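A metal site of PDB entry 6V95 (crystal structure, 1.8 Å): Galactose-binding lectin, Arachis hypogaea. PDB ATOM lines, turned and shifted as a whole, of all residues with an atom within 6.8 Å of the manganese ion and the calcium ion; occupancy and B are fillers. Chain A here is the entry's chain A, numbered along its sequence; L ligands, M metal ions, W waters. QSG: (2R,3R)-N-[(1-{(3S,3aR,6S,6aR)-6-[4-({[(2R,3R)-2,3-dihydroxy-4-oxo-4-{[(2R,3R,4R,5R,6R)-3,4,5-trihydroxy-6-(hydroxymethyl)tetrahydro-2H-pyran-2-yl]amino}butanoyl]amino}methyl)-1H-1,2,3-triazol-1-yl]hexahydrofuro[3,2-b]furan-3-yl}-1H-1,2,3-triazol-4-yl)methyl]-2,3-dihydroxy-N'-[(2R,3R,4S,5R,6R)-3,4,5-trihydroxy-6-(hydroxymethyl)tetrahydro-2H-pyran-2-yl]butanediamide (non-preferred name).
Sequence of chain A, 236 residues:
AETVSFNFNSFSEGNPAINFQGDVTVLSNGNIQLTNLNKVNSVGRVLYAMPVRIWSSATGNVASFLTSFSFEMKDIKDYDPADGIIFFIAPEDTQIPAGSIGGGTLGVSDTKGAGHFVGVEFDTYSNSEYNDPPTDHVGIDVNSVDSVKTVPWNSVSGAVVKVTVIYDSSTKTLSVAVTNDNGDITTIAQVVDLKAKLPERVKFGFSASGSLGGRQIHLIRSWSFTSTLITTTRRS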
ATOM      1  N   ASP A  83       5.647   6.352  -3.775  1.00  0.00           N
ATOM      2  CA  ASP A  83       5.256   5.939  -2.417  1.00  0.00           C
ATOM      3  C   ASP A  83       4.070   4.992  -2.355  1.00  0.00           C
ATOM      4  O   ASP A  83       3.832   4.412  -1.301  1.00  0.00           O
ATOM      5  CB  ASP A  83       4.950   7.161  -1.573  1.00  0.00           C
ATOM      6  CG  ASP A  83       6.208   7.728  -0.977  1.00  0.00           C
ATOM      7  OD1 ASP A  83       6.849   8.593  -1.646  1.00  0.00           O
ATOM      8  OD2 ASP A  83       6.625   7.235   0.090  1.00  0.00           O
ATOM      9  N   GLY A 103       5.002  12.298  -1.118  1.00  0.00           N
ATOM     10  CA  GLY A 103       5.646  11.262  -0.311  1.00  0.00           C
ATOM     11  C   GLY A 103       4.654  10.332   0.403  1.00  0.00           C
ATOM     12  O   GLY A 103       3.752   9.778  -0.237  1.00  0.00           O
ATOM     13  N   GLY A 104       4.849  10.202   1.717  1.00  0.00           N
ATOM     14  CA  GLY A 104       4.054   9.337   2.583  1.00  0.00           C
ATOM     15  C   GLY A 104       2.602   9.747   2.776  1.00  0.00           C
ATOM     16  O   GLY A 104       1.794   8.955   3.273  1.00  0.00           O
ATOM     17  N   THR A 105       2.290  11.004   2.433  1.00  0.00           N
ATOM     18  CA  THR A 105       0.934  11.546   2.533  1.00  0.00           C
ATOM     19  C   THR A 105      -0.015  10.899   1.488  1.00  0.00           C
ATOM     20  O   THR A 105      -1.215  11.085   1.589  1.00  0.00           O
ATOM     21  CB  THR A 105       0.945  13.091   2.369  1.00  0.00           C
ATOM     22  OG1 THR A 105       1.124  13.444   0.996  1.00  0.00           O
ATOM     23  CG2 THR A 105       1.970  13.775   3.277  1.00  0.00           C
ATOM     24  N   LEU A 106       0.546  10.250   0.425  1.00  0.00           N
ATOM     25  CA  LEU A 106      -0.159   9.582  -0.685  1.00  0.00           C
ATOM     26  C   LEU A 106      -1.138  10.541  -1.432  1.00  0.00           C
ATOM     27  O   LEU A 106      -2.049  10.083  -2.144  1.00  0.00           O
ATOM     28  CB  LEU A 106      -0.897   8.305  -0.198  1.00  0.00           C
ATOM     29  CG  LEU A 106      -0.040   7.226   0.457  1.00  0.00           C
ATOM     30  CD1 LEU A 106      -0.910   6.051   0.915  1.00  0.00           C
ATOM     31  CD2 LEU A 106       1.090   6.722  -0.483  1.00  0.00           C
ATOM     32  N   GLU A 121      -5.028   1.870   0.990  1.00  0.00           N
ATOM     33  CA  GLU A 121      -3.713   2.186   0.470  1.00  0.00           C
ATOM     34  C   GLU A 121      -2.903   0.926   0.127  1.00  0.00           C
ATOM     35  O   GLU A 121      -2.994  -0.101   0.814  1.00  0.00           O
ATOM     36  CB  GLU A 121      -2.933   3.051   1.472  1.00  0.00           C
ATOM     37  CG  GLU A 121      -2.808   2.362   2.827  1.00  0.00           C
ATOM     38  CD  GLU A 121      -1.760   3.027   3.668  1.00  0.00           C
ATOM     39  OE1 GLU A 121      -1.917   4.239   3.932  1.00  0.00           O
ATOM     40  OE2 GLU A 121      -0.738   2.378   3.984  1.00  0.00           O
ATOM     41  N   ASP A 123       0.725   0.702  -0.074  1.00  0.00           N
ATOM     42  CA  ASP A 123       1.882   1.463   0.370  1.00  0.00           C
ATOM     43  C   ASP A 123       3.205   0.729   0.173  1.00  0.00           C
ATOM     44  O   ASP A 123       3.373  -0.385   0.672  1.00  0.00           O
ATOM     45  CB  ASP A 123       1.664   1.808   1.840  1.00  0.00           C
ATOM     46  CG  ASP A 123       2.557   2.896   2.370  1.00  0.00           C
ATOM     47  OD1 ASP A 123       3.537   3.280   1.674  1.00  0.00           O
ATOM     48  OD2 ASP A 123       2.283   3.391   3.477  1.00  0.00           O
ATOM     49  N   THR A 124       4.156   1.363  -0.580  1.00  0.00           N
ATOM     50  CA  THR A 124       5.428   0.725  -0.940  1.00  0.00           C
ATOM     51  C   THR A 124       6.664   1.351  -0.262  1.00  0.00           C
ATOM     52  O   THR A 124       7.796   1.018  -0.647  1.00  0.00           O
ATOM     53  CB  THR A 124       5.586   0.725  -2.465  1.00  0.00           C
ATOM     54  OG1 THR A 124       5.938   2.035  -2.914  1.00  0.00           O
ATOM     55  CG2 THR A 124       4.335   0.256  -3.196  1.00  0.00           C
ATOM     56  N   TYR A 125       6.475   2.192   0.772  1.00  0.00           N
ATOM     57  CA  TYR A 125       7.583   2.833   1.508  1.00  0.00           C
ATOM     58  C   TYR A 125       7.189   3.021   2.970  1.00  0.00           C
ATOM     59  O   TYR A 125       6.110   3.565   3.247  1.00  0.00           O
ATOM     60  CB  TYR A 125       8.006   4.172   0.890  1.00  0.00           C
ATOM     61  CG  TYR A 125       9.232   4.738   1.587  1.00  0.00           C
ATOM     62  CD1 TYR A 125      10.515   4.374   1.178  1.00  0.00           C
ATOM     63  CD2 TYR A 125       9.109   5.564   2.700  1.00  0.00           C
ATOM     64  CE1 TYR A 125      11.638   4.876   1.836  1.00  0.00           C
ATOM     65  CE2 TYR A 125      10.222   6.004   3.400  1.00  0.00           C
ATOM     66  CZ  TYR A 125      11.485   5.655   2.967  1.00  0.00           C
ATOM     67  OH  TYR A 125      12.604   6.127   3.623  1.00  0.00           O
ATOM     68  N   SER A 126       8.060   2.593   3.903  1.00  0.00           N
ATOM     69  CA  SER A 126       7.784   2.655   5.344  1.00  0.00           C
ATOM     70  C   SER A 126       8.120   4.031   5.929  1.00  0.00           C
ATOM     71  O   SER A 126       9.293   4.372   6.075  1.00  0.00           O
ATOM     72  CB  SER A 126       8.535   1.556   6.085  1.00  0.00           C
ATOM     73  OG  SER A 126       8.184   1.510   7.459  1.00  0.00           O
ATOM     74  N   ASN A 127       7.072   4.823   6.210  1.00  0.00           N
ATOM     75  CA  ASN A 127       7.156   6.154   6.811  1.00  0.00           C
ATOM     76  C   ASN A 127       6.992   6.044   8.326  1.00  0.00           C
ATOM     77  O   ASN A 127       5.865   5.946   8.812  1.00  0.00           O
ATOM     78  CB  ASN A 127       6.113   7.094   6.220  1.00  0.00           C
ATOM     79  CG  ASN A 127       6.297   7.360   4.759  1.00  0.00           C
ATOM     80  OD1 ASN A 127       5.991   6.531   3.896  1.00  0.00           O
ATOM     81  ND2 ASN A 127       6.767   8.555   4.432  1.00  0.00           N
ATOM     82  N   TYR A 130       4.429   8.141  10.147  1.00  0.00           N
ATOM     83  CA  TYR A 130       3.017   7.731  10.052  1.00  0.00           C
ATOM     84  C   TYR A 130       2.788   6.315  10.632  1.00  0.00           C
ATOM     85  O   TYR A 130       1.756   5.698  10.381  1.00  0.00           O
ATOM     86  CB  TYR A 130       2.521   7.800   8.598  1.00  0.00           C
ATOM     87  CG  TYR A 130       2.756   9.148   7.952  1.00  0.00           C
ATOM     88  CD1 TYR A 130       2.448  10.328   8.628  1.00  0.00           C
ATOM     89  CD2 TYR A 130       3.271   9.256   6.658  1.00  0.00           C
ATOM     90  CE1 TYR A 130       2.678  11.571   8.049  1.00  0.00           C
ATOM     91  CE2 TYR A 130       3.528  10.495   6.089  1.00  0.00           C
ATOM     92  CZ  TYR A 130       3.224  11.644   6.781  1.00  0.00           C
ATOM     93  OH  TYR A 130       3.442  12.868   6.205  1.00  0.00           O
ATOM     94  N   ASN A 131       3.763   5.839  11.437  1.00  0.00           N
ATOM     95  CA  ASN A 131       3.771   4.527  12.102  1.00  0.00           C
ATOM     96  C   ASN A 131       3.528   3.372  11.098  1.00  0.00           C
ATOM     97  O   ASN A 131       2.843   2.400  11.423  1.00  0.00           O
ATOM     98  CB  ASN A 131       2.757   4.496  13.270  1.00  0.00           C
ATOM     99  CG  ASN A 131       3.130   5.433  14.402  1.00  0.00           C
ATOM    100  OD1 ASN A 131       4.234   5.366  14.969  1.00  0.00           O
ATOM    101  ND2 ASN A 131       2.222   6.333  14.745  1.00  0.00           N
ATOM    102  N   ASP A 132       4.119   3.495   9.894  1.00  0.00           N
ATOM    103  CA  ASP A 132       4.007   2.455   8.857  1.00  0.00           C
ATOM    104  C   ASP A 132       4.622   1.138   9.325  1.00  0.00           C
ATOM    105  O   ASP A 132       5.670   1.185   9.985  1.00  0.00           O
ATOM    106  CB  ASP A 132       4.717   2.879   7.570  1.00  0.00           C
ATOM    107  CG  ASP A 132       3.858   3.574   6.543  1.00  0.00           C
ATOM    108  OD1 ASP A 132       2.627   3.403   6.594  1.00  0.00           O
ATOM    109  OD2 ASP A 132       4.414   4.252   5.659  1.00  0.00           O
ATOM    110  N   PRO A 133       4.095  -0.029   8.924  1.00  0.00           N
ATOM    111  CA  PRO A 133       4.772  -1.290   9.295  1.00  0.00           C
ATOM    112  C   PRO A 133       6.111  -1.388   8.520  1.00  0.00           C
ATOM    113  O   PRO A 133       6.303  -0.615   7.585  1.00  0.00           O
ATOM    114  CB  PRO A 133       3.763  -2.380   8.925  1.00  0.00           C
ATOM    115  CG  PRO A 133       2.868  -1.762   7.915  1.00  0.00           C
ATOM    116  CD  PRO A 133       2.850  -0.285   8.150  1.00  0.00           C
ATOM    117  N   HIS A 137       2.651  -2.864   2.382  1.00  0.00           N
ATOM    118  CA  HIS A 137       1.399  -3.237   3.032  1.00  0.00           C
ATOM    119  C   HIS A 137       0.166  -2.630   2.376  1.00  0.00           C
ATOM    120  O   HIS A 137       0.248  -1.603   1.693  1.00  0.00           O
ATOM    121  CB  HIS A 137       1.448  -2.790   4.531  1.00  0.00           C
ATOM    122  CG  HIS A 137       1.764  -1.337   4.706  1.00  0.00           C
ATOM    123  ND1 HIS A 137       3.078  -0.840   4.580  1.00  0.00           N
ATOM    124  CD2 HIS A 137       0.938  -0.303   4.975  1.00  0.00           C
ATOM    125  CE1 HIS A 137       2.981   0.458   4.784  1.00  0.00           C
ATOM    126  NE2 HIS A 137       1.715   0.827   5.034  1.00  0.00           N
ATOM    127  N   VAL A 138      -0.964  -3.291   2.611  1.00  0.00           N
ATOM    128  CA  VAL A 138      -2.287  -2.799   2.254  1.00  0.00           C
ATOM    129  C   VAL A 138      -2.848  -2.285   3.552  1.00  0.00           C
ATOM    130  O   VAL A 138      -2.755  -2.961   4.584  1.00  0.00           O
ATOM    131  CB  VAL A 138      -3.198  -3.845   1.550  1.00  0.00           C
ATOM    132  CG1 VAL A 138      -4.559  -3.237   1.201  1.00  0.00           C
ATOM    133  CG2 VAL A 138      -2.534  -4.417   0.299  1.00  0.00           C
ATOM    134  N   GLY A 139      -3.338  -1.060   3.534  1.00  0.00           N
ATOM    135  CA  GLY A 139      -3.900  -0.459   4.734  1.00  0.00           C
ATOM    136  C   GLY A 139      -5.297   0.075   4.545  1.00  0.00           C
ATOM    137  O   GLY A 139      -5.698   0.415   3.432  1.00  0.00           O
ATOM    138  N   ASP A 141      -7.542   3.128   5.814  1.00  0.00           N
ATOM    139  CA  ASP A 141      -7.311   4.473   6.321  1.00  0.00           C
ATOM    140  C   ASP A 141      -8.597   5.230   6.569  1.00  0.00           C
ATOM    141  O   ASP A 141      -9.496   5.252   5.733  1.00  0.00           O
ATOM    142  CB  ASP A 141      -6.456   5.266   5.310  1.00  0.00           C
ATOM    143  CG  ASP A 141      -5.041   4.762   5.111  1.00  0.00           C
ATOM    144  OD1 ASP A 141      -4.634   3.844   5.848  1.00  0.00           O
ATOM    145  OD2 ASP A 141      -4.358   5.280   4.208  1.00  0.00           O
ATOM    146  N   VAL A 145      -3.194   8.713   7.195  1.00  0.00           N
ATOM    147  CA  VAL A 145      -2.308   7.752   6.547  1.00  0.00           C
ATOM    148  C   VAL A 145      -1.600   6.903   7.644  1.00  0.00           C
ATOM    149  O   VAL A 145      -0.811   6.009   7.330  1.00  0.00           O
ATOM    150  CB  VAL A 145      -1.317   8.346   5.498  1.00  0.00           C
ATOM    151  CG1 VAL A 145      -2.065   8.874   4.272  1.00  0.00           C
ATOM    152  CG2 VAL A 145      -0.417   9.409   6.099  1.00  0.00           C
ATOM    153  N   ASP A 146      -1.937   7.153   8.946  1.00  0.00           N
ATOM    154  CA  ASP A 146      -1.561   6.261  10.028  1.00  0.00           C
ATOM    155  C   ASP A 146      -2.733   5.283  10.080  1.00  0.00           C
ATOM    156  O   ASP A 146      -3.763   5.557  10.710  1.00  0.00           O
ATOM    157  CB  ASP A 146      -1.318   7.024  11.359  1.00  0.00           C
ATOM    158  CG  ASP A 146      -0.801   6.168  12.526  1.00  0.00           C
ATOM    159  OD1 ASP A 146      -0.967   4.919  12.485  1.00  0.00           O
ATOM    160  OD2 ASP A 146      -0.257   6.735  13.496  1.00  0.00           O
ATOM    161  N   SER A 147      -2.637   4.221   9.268  1.00  0.00           N
ATOM    162  CA  SER A 147      -3.725   3.265   9.057  1.00  0.00           C
ATOM    163  C   SER A 147      -4.371   2.720  10.346  1.00  0.00           C
ATOM    164  O   SER A 147      -3.692   2.426  11.355  1.00  0.00           O
ATOM    165  CB  SER A 147      -3.260   2.081   8.215  1.00  0.00           C
ATOM    166  OG  SER A 147      -2.696   2.444   6.962  1.00  0.00           O
ATOM    167  N   THR A 150      -3.416  -2.589   8.933  1.00  0.00           N
ATOM    168  CA  THR A 150      -2.607  -2.965   7.784  1.00  0.00           C
ATOM    169  C   THR A 150      -2.457  -4.471   7.730  1.00  0.00           C
ATOM    170  O   THR A 150      -2.660  -5.165   8.744  1.00  0.00           O
ATOM    171  CB  THR A 150      -1.198  -2.296   7.779  1.00  0.00           C
ATOM    172  OG1 THR A 150      -0.385  -2.843   8.810  1.00  0.00           O
ATOM    173  CG2 THR A 150      -1.234  -0.787   7.839  1.00  0.00           C
HETATM  174  N1  QSG L   1      11.901  11.584   2.251  1.00  0.00           N
HETATM  175  C4  QSG L   1       9.684   8.404   0.516  1.00  0.00           C
HETATM  176  C3  QSG L   1       9.063   9.177   1.684  1.00  0.00           C
HETATM  177  C5  QSG L   1      11.212   8.411   0.656  1.00  0.00           C
HETATM  178  C1  QSG L   1      11.215  10.347   2.052  1.00  0.00           C
HETATM  179  C2  QSG L   1       9.697  10.527   1.984  1.00  0.00           C
HETATM  180  C6  QSG L   1      11.952   7.833  -0.519  1.00  0.00           C
HETATM  181  C7  QSG L   1      13.069  11.644   2.904  1.00  0.00           C
HETATM  182  C8  QSG L   1      13.662  13.020   3.202  1.00  0.00           C
HETATM  183  C9  QSG L   1      15.109  13.064   2.681  1.00  0.00           C
HETATM  184  C10 QSG L   1      15.930  14.034   3.525  1.00  0.00           C
HETATM  185  O5  QSG L   1      11.679   9.751   0.830  1.00  0.00           O
HETATM  186  O2  QSG L   1       9.219  11.033   3.224  1.00  0.00           O
HETATM  187  O3  QSG L   1       7.637   9.208   1.690  1.00  0.00           O
HETATM  188  O4  QSG L   1       9.359   8.965  -0.758  1.00  0.00           O
HETATM  189  O6  QSG L   1      13.295   7.471  -0.177  1.00  0.00           O
HETATM  190  O10 QSG L   1      15.907  13.960   4.753  1.00  0.00           O
HETATM  191  O9  QSG L   1      15.159  13.396   1.296  1.00  0.00           O
HETATM  192  O8  QSG L   1      12.880  14.062   2.653  1.00  0.00           O
HETATM  193  O7  QSG L   1      13.676  10.647   3.271  1.00  0.00           O
HETATM  194 MN    MN M   1       1.129   2.793   5.198  1.00  0.00          MN
HETATM  195 CA    CA M   2       4.323   4.815   3.376  1.00  0.00          CA
HETATM  196  O   HOH W   1       4.519   5.780   1.311  1.00  0.00           O
HETATM  197  O   HOH W   2       2.506   6.444   3.857  1.00  0.00           O
HETATM  198  O   HOH W   3       0.061   2.255   6.922  1.00  0.00           O
HETATM  199  O   HOH W   4       0.359   5.032   5.123  1.00  0.00           O
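The side-chain amide nitrogen (ND2) of Asn 127 sits at hydrogen-bond distance from an oxygen (O3) of the ligand.
The backbone NH of Gly 104 is in hydrogen-bond range of an oxygen (O3) of the ligand (3.0 Å).
OD1 of Asp 83 is in hydrogen-bond range of O4 of the ligand, at 2.7 Å.
The manganese ion is bound by NE2 of His 137 (2.1 Å), water W3 (2.1 Å), OD1 of Asp 132 (2.1 Å), OD2 of Asp 123 (2.2 Å), OE2 of Glu 121 (2.3 Å) and water W4 (2.4 Å).
Water W4 bridges O of Val 145 and OE1 of Glu 121.
The side-chain carboxylate of Glu 121 sits close to the side-chain carboxylate of Asp 141.
O of Glu 121 lies within hydrogen-bond range of N of Gly 139, 2.9 Å away.
Of the 23 residues printed, 4 come within 4 Å of the manganese ion.
The nearest printed residue that does not touch the manganese ion is Ser 147 (4.2 Å).
The calcium ion is bound by O of Tyr 125, water W1, OD2 of Asp 132, OD1 of Asp 123, OD1 of Asn 127, water W2 and OD2 of Asp 123.
The calcium ion has seven donor atoms within binding distance.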
